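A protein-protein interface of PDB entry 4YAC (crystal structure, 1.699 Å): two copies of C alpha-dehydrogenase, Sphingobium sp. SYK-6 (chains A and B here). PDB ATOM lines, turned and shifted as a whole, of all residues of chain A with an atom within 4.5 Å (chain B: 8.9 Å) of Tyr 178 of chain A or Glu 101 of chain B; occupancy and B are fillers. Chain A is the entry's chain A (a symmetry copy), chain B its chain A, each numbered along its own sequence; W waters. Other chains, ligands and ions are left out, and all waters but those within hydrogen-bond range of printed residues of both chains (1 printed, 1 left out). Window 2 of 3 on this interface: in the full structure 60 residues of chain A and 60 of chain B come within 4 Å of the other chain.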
ATOM      1  N   MET A 127      -5.390  26.481 -28.389  1.00  0.00           N
ATOM      2  CA  MET A 127      -5.326  25.023 -28.343  1.00  0.00           C
ATOM      3  C   MET A 127      -5.493  24.372 -29.727  1.00  0.00           C
ATOM      4  O   MET A 127      -4.796  23.402 -30.039  1.00  0.00           O
ATOM      5  CB  MET A 127      -6.372  24.502 -27.349  1.00  0.00           C
ATOM      6  CG  MET A 127      -6.593  23.008 -27.344  1.00  0.00           C
ATOM      7  SD  MET A 127      -8.041  22.562 -28.317  1.00  0.00           S
ATOM      8  CE  MET A 127      -9.373  23.366 -27.416  1.00  0.00           C
ATOM      9  N   PRO A 128      -6.392  24.904 -30.574  1.00  0.00           N
ATOM     10  CA  PRO A 128      -6.463  24.349 -31.934  1.00  0.00           C
ATOM     11  C   PRO A 128      -5.187  24.556 -32.759  1.00  0.00           C
ATOM     12  O   PRO A 128      -4.893  23.751 -33.645  1.00  0.00           O
ATOM     13  CB  PRO A 128      -7.640  25.103 -32.557  1.00  0.00           C
ATOM     14  CG  PRO A 128      -8.500  25.463 -31.393  1.00  0.00           C
ATOM     15  CD  PRO A 128      -7.536  25.789 -30.290  1.00  0.00           C
ATOM     16  N   ILE A 131      -2.722  21.782 -31.595  1.00  0.00           N
ATOM     17  CA  ILE A 131      -3.070  20.495 -32.188  1.00  0.00           C
ATOM     18  C   ILE A 131      -2.619  20.448 -33.643  1.00  0.00           C
ATOM     19  O   ILE A 131      -2.009  19.471 -34.086  1.00  0.00           O
ATOM     20  CB  ILE A 131      -4.598  20.232 -32.078  1.00  0.00           C
ATOM     21  CG1 ILE A 131      -4.963  19.964 -30.618  1.00  0.00           C
ATOM     22  CG2 ILE A 131      -5.022  19.049 -32.942  1.00  0.00           C
ATOM     23  CD1 ILE A 131      -6.441  19.968 -30.337  1.00  0.00           C
ATOM     24  N   GLY A 136       2.815  19.169 -29.501  1.00  0.00           N
ATOM     25  CA  GLY A 136       2.389  19.189 -28.117  1.00  0.00           C
ATOM     26  C   GLY A 136       2.268  20.603 -27.588  1.00  0.00           C
ATOM     27  O   GLY A 136       2.240  21.570 -28.350  1.00  0.00           O
ATOM     28  N   GLU A 174      -9.220  15.297 -22.776  1.00  0.00           N
ATOM     29  CA  GLU A 174      -9.099  15.273 -24.232  1.00  0.00           C
ATOM     30  C   GLU A 174      -7.729  15.695 -24.767  1.00  0.00           C
ATOM     31  O   GLU A 174      -7.400  15.391 -25.914  1.00  0.00           O
ATOM     32  CB  GLU A 174     -10.189  16.161 -24.846  1.00  0.00           C
ATOM     33  CG  GLU A 174     -11.601  15.663 -24.527  1.00  0.00           C
ATOM     34  CD  GLU A 174     -12.698  16.401 -25.273  1.00  0.00           C
ATOM     35  OE1 GLU A 174     -12.482  16.807 -26.433  1.00  0.00           O
ATOM     36  OE2 GLU A 174     -13.794  16.560 -24.699  1.00  0.00           O
ATOM     37  N   MET A 175      -6.924  16.373 -23.956  1.00  0.00           N
ATOM     38  CA  MET A 175      -5.655  16.916 -24.451  1.00  0.00           C
ATOM     39  C   MET A 175      -4.466  15.937 -24.471  1.00  0.00           C
ATOM     40  O   MET A 175      -3.577  16.081 -25.312  1.00  0.00           O
ATOM     41  CB  MET A 175      -5.276  18.150 -23.634  1.00  0.00           C
ATOM     42  CG  MET A 175      -6.168  19.362 -23.898  1.00  0.00           C
ATOM     43  SD  MET A 175      -6.182  19.887 -25.632  1.00  0.00           S
ATOM     44  CE  MET A 175      -7.694  19.118 -26.209  1.00  0.00           C
ATOM     45  N   PRO A 176      -4.431  14.948 -23.560  1.00  0.00           N
ATOM     46  CA  PRO A 176      -3.260  14.058 -23.567  1.00  0.00           C
ATOM     47  C   PRO A 176      -3.009  13.315 -24.883  1.00  0.00           C
ATOM     48  O   PRO A 176      -1.849  13.057 -25.196  1.00  0.00           O
ATOM     49  CB  PRO A 176      -3.577  13.067 -22.449  1.00  0.00           C
ATOM     50  CG  PRO A 176      -4.413  13.843 -21.507  1.00  0.00           C
ATOM     51  CD  PRO A 176      -5.272  14.722 -22.371  1.00  0.00           C
ATOM     52  N   LYS A 177      -4.049  12.989 -25.643  1.00  0.00           N
ATOM     53  CA  LYS A 177      -3.846  12.284 -26.907  1.00  0.00           C
ATOM     54  C   LYS A 177      -3.165  13.178 -27.951  1.00  0.00           C
ATOM     55  O   LYS A 177      -2.692  12.689 -28.976  1.00  0.00           O
ATOM     56  CB  LYS A 177      -5.174  11.748 -27.452  1.00  0.00           C
ATOM     57  CG  LYS A 177      -6.216  12.798 -27.785  1.00  0.00           C
ATOM     58  CD  LYS A 177      -7.462  12.145 -28.372  1.00  0.00           C
ATOM     59  CE  LYS A 177      -8.508  13.170 -28.783  1.00  0.00           C
ATOM     60  NZ  LYS A 177      -8.988  13.986 -27.632  1.00  0.00           N
ATOM     61  N   TYR A 178      -3.112  14.481 -27.678  1.00  0.00           N
ATOM     62  CA  TYR A 178      -2.394  15.434 -28.527  1.00  0.00           C
ATOM     63  C   TYR A 178      -1.076  15.874 -27.892  1.00  0.00           C
ATOM     64  O   TYR A 178      -0.443  16.822 -28.362  1.00  0.00           O
ATOM     65  CB  TYR A 178      -3.255  16.665 -28.805  1.00  0.00           C
ATOM     66  CG  TYR A 178      -4.536  16.372 -29.549  1.00  0.00           C
ATOM     67  CD1 TYR A 178      -4.512  15.802 -30.814  1.00  0.00           C
ATOM     68  CD2 TYR A 178      -5.769  16.685 -28.997  1.00  0.00           C
ATOM     69  CE1 TYR A 178      -5.679  15.538 -31.502  1.00  0.00           C
ATOM     70  CE2 TYR A 178      -6.940  16.427 -29.677  1.00  0.00           C
ATOM     71  CZ  TYR A 178      -6.892  15.855 -30.929  1.00  0.00           C
ATOM     72  OH  TYR A 178      -8.058  15.596 -31.607  1.00  0.00           O
ATOM     73  N   ASN A 179      -0.679  15.188 -26.823  1.00  0.00           N
ATOM     74  CA  ASN A 179       0.532  15.522 -26.081  1.00  0.00           C
ATOM     75  C   ASN A 179       0.490  16.955 -25.558  1.00  0.00           C
ATOM     76  O   ASN A 179       1.512  17.641 -25.501  1.00  0.00           O
ATOM     77  CB  ASN A 179       1.773  15.306 -26.952  1.00  0.00           C
ATOM     78  CG  ASN A 179       1.985  13.846 -27.304  1.00  0.00           C
ATOM     79  OD1 ASN A 179       1.719  12.957 -26.493  1.00  0.00           O
ATOM     80  ND2 ASN A 179       2.461  13.589 -28.517  1.00  0.00           N
ATOM     81  N   ILE A 180      -0.706  17.393 -25.172  1.00  0.00           N
ATOM     82  CA  ILE A 180      -0.894  18.702 -24.563  1.00  0.00           C
ATOM     83  C   ILE A 180      -1.233  18.518 -23.085  1.00  0.00           C
ATOM     84  O   ILE A 180      -2.266  17.945 -22.740  1.00  0.00           O
ATOM     85  CB  ILE A 180      -2.002  19.511 -25.280  1.00  0.00           C
ATOM     86  CG1 ILE A 180      -1.566  19.843 -26.710  1.00  0.00           C
ATOM     87  CG2 ILE A 180      -2.320  20.801 -24.513  1.00  0.00           C
ATOM     88  CD1 ILE A 180      -2.666  20.421 -27.581  1.00  0.00           C
ATOM     89  N   GLY B  98     -19.145  17.103 -28.580  1.00  0.00           N
ATOM     90  CA  GLY B  98     -18.185  17.011 -29.663  1.00  0.00           C
ATOM     91  C   GLY B  98     -16.784  17.256 -29.142  1.00  0.00           C
ATOM     92  O   GLY B  98     -16.620  17.739 -28.025  1.00  0.00           O
ATOM     93  N   PRO B  99     -15.765  16.923 -29.946  1.00  0.00           N
ATOM     94  CA  PRO B  99     -14.380  17.188 -29.538  1.00  0.00           C
ATOM     95  C   PRO B  99     -14.206  18.653 -29.186  1.00  0.00           C
ATOM     96  O   PRO B  99     -14.691  19.500 -29.934  1.00  0.00           O
ATOM     97  CB  PRO B  99     -13.558  16.826 -30.779  1.00  0.00           C
ATOM     98  CG  PRO B  99     -14.447  15.963 -31.602  1.00  0.00           C
ATOM     99  CD  PRO B  99     -15.848  16.387 -31.315  1.00  0.00           C
ATOM    100  N   ILE B 100     -13.545  18.955 -28.077  1.00  0.00           N
ATOM    101  CA  ILE B 100     -13.481  20.336 -27.619  1.00  0.00           C
ATOM    102  C   ILE B 100     -12.731  21.208 -28.625  1.00  0.00           C
ATOM    103  O   ILE B 100     -13.012  22.398 -28.741  1.00  0.00           O
ATOM    104  CB  ILE B 100     -12.812  20.453 -26.227  1.00  0.00           C
ATOM    105  CG1 ILE B 100     -12.905  21.888 -25.692  1.00  0.00           C
ATOM    106  CG2 ILE B 100     -11.357  20.023 -26.280  1.00  0.00           C
ATOM    107  CD1 ILE B 100     -14.310  22.450 -25.619  1.00  0.00           C
ATOM    108  N   GLU B 101     -11.801  20.617 -29.370  1.00  0.00           N
ATOM    109  CA  GLU B 101     -11.006  21.396 -30.313  1.00  0.00           C
ATOM    110  C   GLU B 101     -11.806  21.784 -31.560  1.00  0.00           C
ATOM    111  O   GLU B 101     -11.357  22.616 -32.349  1.00  0.00           O
ATOM    112  CB  GLU B 101      -9.739  20.632 -30.717  1.00  0.00           C
ATOM    113  CG  GLU B 101      -9.957  19.402 -31.603  1.00  0.00           C
ATOM    114  CD  GLU B 101     -10.116  18.112 -30.821  1.00  0.00           C
ATOM    115  OE1 GLU B 101     -10.351  18.169 -29.596  1.00  0.00           O
ATOM    116  OE2 GLU B 101     -10.000  17.032 -31.441  1.00  0.00           O
ATOM    117  N   LYS B 102     -12.976  21.176 -31.739  1.00  0.00           N
ATOM    118  CA  LYS B 102     -13.850  21.494 -32.873  1.00  0.00           C
ATOM    119  C   LYS B 102     -15.032  22.375 -32.468  1.00  0.00           C
ATOM    120  O   LYS B 102     -15.860  22.725 -33.305  1.00  0.00           O
ATOM    121  CB  LYS B 102     -14.383  20.215 -33.531  1.00  0.00           C
ATOM    122  CG  LYS B 102     -13.317  19.320 -34.162  1.00  0.00           C
ATOM    123  CD  LYS B 102     -12.403  20.078 -35.118  1.00  0.00           C
ATOM    124  CE  LYS B 102     -11.383  19.150 -35.758  1.00  0.00           C
ATOM    125  NZ  LYS B 102     -10.257  19.904 -36.378  1.00  0.00           N
ATOM    126  N   ALA B 103     -15.108  22.732 -31.189  1.00  0.00           N
ATOM    127  CA  ALA B 103     -16.194  23.580 -30.706  1.00  0.00           C
ATOM    128  C   ALA B 103     -16.078  24.976 -31.306  1.00  0.00           C
ATOM    129  O   ALA B 103     -14.973  25.497 -31.468  1.00  0.00           O
ATOM    130  CB  ALA B 103     -16.178  23.652 -29.187  1.00  0.00           C
ATOM    131  N   THR B 104     -17.219  25.568 -31.656  1.00  0.00           N
ATOM    132  CA  THR B 104     -17.255  26.937 -32.160  1.00  0.00           C
ATOM    133  C   THR B 104     -17.623  27.875 -31.025  1.00  0.00           C
ATOM    134  O   THR B 104     -18.097  27.434 -29.980  1.00  0.00           O
ATOM    135  CB  THR B 104     -18.266  27.113 -33.316  1.00  0.00           C
ATOM    136  OG1 THR B 104     -19.605  26.999 -32.818  1.00  0.00           O
ATOM    137  CG2 THR B 104     -18.031  26.074 -34.403  1.00  0.00           C
ATOM    138  N   ASP B 107     -21.195  27.545 -30.402  1.00  0.00           N
ATOM    139  CA  ASP B 107     -21.487  26.372 -29.574  1.00  0.00           C
ATOM    140  C   ASP B 107     -21.371  26.731 -28.095  1.00  0.00           C
ATOM    141  O   ASP B 107     -22.236  26.390 -27.288  1.00  0.00           O
ATOM    142  CB  ASP B 107     -20.539  25.203 -29.882  1.00  0.00           C
ATOM    143  CG  ASP B 107     -20.747  24.610 -31.264  1.00  0.00           C
ATOM    144  OD1 ASP B 107     -21.866  24.720 -31.807  1.00  0.00           O
ATOM    145  OD2 ASP B 107     -19.779  24.012 -31.797  1.00  0.00           O
ATOM    146  N   TRP B 108     -20.279  27.409 -27.750  1.00  0.00           N
ATOM    147  CA  TRP B 108     -20.045  27.848 -26.380  1.00  0.00           C
ATOM    148  C   TRP B 108     -21.138  28.796 -25.890  1.00  0.00           C
ATOM    149  O   TRP B 108     -21.727  28.587 -24.824  1.00  0.00           O
ATOM    150  CB  TRP B 108     -18.685  28.541 -26.270  1.00  0.00           C
ATOM    151  CG  TRP B 108     -17.532  27.621 -26.000  1.00  0.00           C
ATOM    152  CD1 TRP B 108     -16.562  27.230 -26.883  1.00  0.00           C
ATOM    153  CD2 TRP B 108     -17.205  27.004 -24.751  1.00  0.00           C
ATOM    154  NE1 TRP B 108     -15.666  26.398 -26.260  1.00  0.00           N
ATOM    155  CE2 TRP B 108     -16.040  26.244 -24.949  1.00  0.00           C
ATOM    156  CE3 TRP B 108     -17.794  27.012 -23.481  1.00  0.00           C
ATOM    157  CZ2 TRP B 108     -15.449  25.501 -23.932  1.00  0.00           C
ATOM    158  CZ3 TRP B 108     -17.202  26.270 -22.474  1.00  0.00           C
ATOM    159  CH2 TRP B 108     -16.046  25.527 -22.705  1.00  0.00           C
ATOM    160  N   THR B 153     -15.808  14.610 -25.038  1.00  0.00           N
ATOM    161  CA  THR B 153     -16.795  15.309 -25.872  1.00  0.00           C
ATOM    162  C   THR B 153     -17.844  16.123 -25.107  1.00  0.00           C
ATOM    163  O   THR B 153     -18.699  16.749 -25.736  1.00  0.00           O
ATOM    164  CB  THR B 153     -17.573  14.337 -26.814  1.00  0.00           C
ATOM    165  OG1 THR B 153     -18.599  13.647 -26.090  1.00  0.00           O
ATOM    166  CG2 THR B 153     -16.634  13.337 -27.497  1.00  0.00           C
ATOM    167  N   GLY B 155     -17.119  18.706 -23.022  1.00  0.00           N
ATOM    168  CA  GLY B 155     -16.382  19.842 -22.490  1.00  0.00           C
ATOM    169  C   GLY B 155     -17.208  21.080 -22.184  1.00  0.00           C
ATOM    170  O   GLY B 155     -17.127  21.632 -21.086  1.00  0.00           O
ATOM    171  N   ILE B 156     -17.994  21.533 -23.155  1.00  0.00           N
ATOM    172  CA  ILE B 156     -18.835  22.709 -22.954  1.00  0.00           C
ATOM    173  C   ILE B 156     -19.891  22.416 -21.897  1.00  0.00           C
ATOM    174  O   ILE B 156     -20.026  23.160 -20.929  1.00  0.00           O
ATOM    175  CB  ILE B 156     -19.519  23.156 -24.262  1.00  0.00           C
ATOM    176  CG1 ILE B 156     -18.463  23.579 -25.289  1.00  0.00           C
ATOM    177  CG2 ILE B 156     -20.472  24.315 -23.993  1.00  0.00           C
ATOM    178  CD1 ILE B 156     -19.029  23.977 -26.636  1.00  0.00           C
HETATM  179  O   HOH W   1     -10.855  15.965 -28.378  1.00  0.00           O
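Printed residues of chain B within 4 Å of Met 127 of chain A: Ile 100 and Glu 101.
Of the printed residues of chain B, Glu 174 of chain A touches Pro 99 (3.7 Å), Ile 100 (2.9 Å) and Thr 153 (2.8 Å).
No residue of chain B comes within 4 Å of Lys 177 of chain A.
Of chain B, only Glu 101 (2.4 Å) comes within 4 Å of Tyr 178 of chain A.
No residue of chain B comes within 4 Å of Asn 179 of chain A.
Printed residues of chain A within 4 Å of Ile 100 of chain B: Met 127, Glu 174 and Met 175.
Of chain A, only Met 127 (3.5 Å), Ile 131 (3.4 Å) and Tyr 178 (2.4 Å) come within 4 Å of Glu 101 of chain B.
The nearest residue of chain B that does not touch Tyr 178 of chain A is Pro 99 of chain B (5.7 Å).
The nearest residue of chain A that does not touch Glu 101 of chain B is Glu 174 of chain A (4.05 Å).
The backbone carbonyl oxygen of Met 175 of chain A sits at hydrogen-bond distance from the backbone NH of Ile 180 of chain A (3.2 Å).
The side-chain amino group of Lys 177 of chain A lies within hydrogen-bond range of the backbone carbonyl oxygen of Glu 174 of chain A.
The backbone NH (N) of Gly 98 of chain B lies within hydrogen-bond range of the backbone carbonyl oxygen (O) of Thr 153 of chain B, at 2.9 Å.
Of the 11 printed residues of chain A, 5 touch a printed residue of chain B.
Hydrophobic or aromatic side chains of chain B that line the printed part of chain A: Ile 100.
Along chain B the printed residues that touch a printed residue of chain A span positions 99 to 153.
Among the printed residues, 8 pairs touch across the chains.
Among the printed residues, no Asp or Glu carboxylate lies within 4 Å of a Lys or Arg side-chain nitrogen of the other chain.
Water W1 lies within hydrogen-bond range of the side-chain carboxylate (OE1) of Glu 101 of chain B (2.6 Å), the side-chain carboxylate (OE1) of Glu 174 of chain A (2.7 Å) and the side-chain amino group (NZ) of Lys 177 of chain A (2.8 Å).
No position is printed for both chains.
Of the 8 pairs that touch across the chains among the printed residues, none has its exchanged pair printed and touching as well.
Among the printed residues, pairs that only touch across the chains: Ile 131 of chain A with Glu 101 of chain B (3.4 Å), Met 127 of chain A with Glu 101 of chain B (3.5 Å), Glu 174 of chain A with Pro 99 of chain B (3.7 Å), Met 175 of chain A with Ile 100 of chain B (3.8 Å) and Met 127 of chain A with Ile 100 of chain B (3.99 Å).
The side-chain hydroxyl (OH) of Tyr 178 of chain A is in hydrogen-bond range of the side-chain carboxylate (OE2) of Glu 101 of chain B (2.4 Å).
The backbone NH of Thr 153 of chain B sits at hydrogen-bond distance from the side-chain carboxylate of Glu 174 of chain A, at 2.8 Å.
OE1 of Glu 174 of chain A lies within hydrogen-bond range of N of Ile 100 of chain B, 2.9 Å away.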
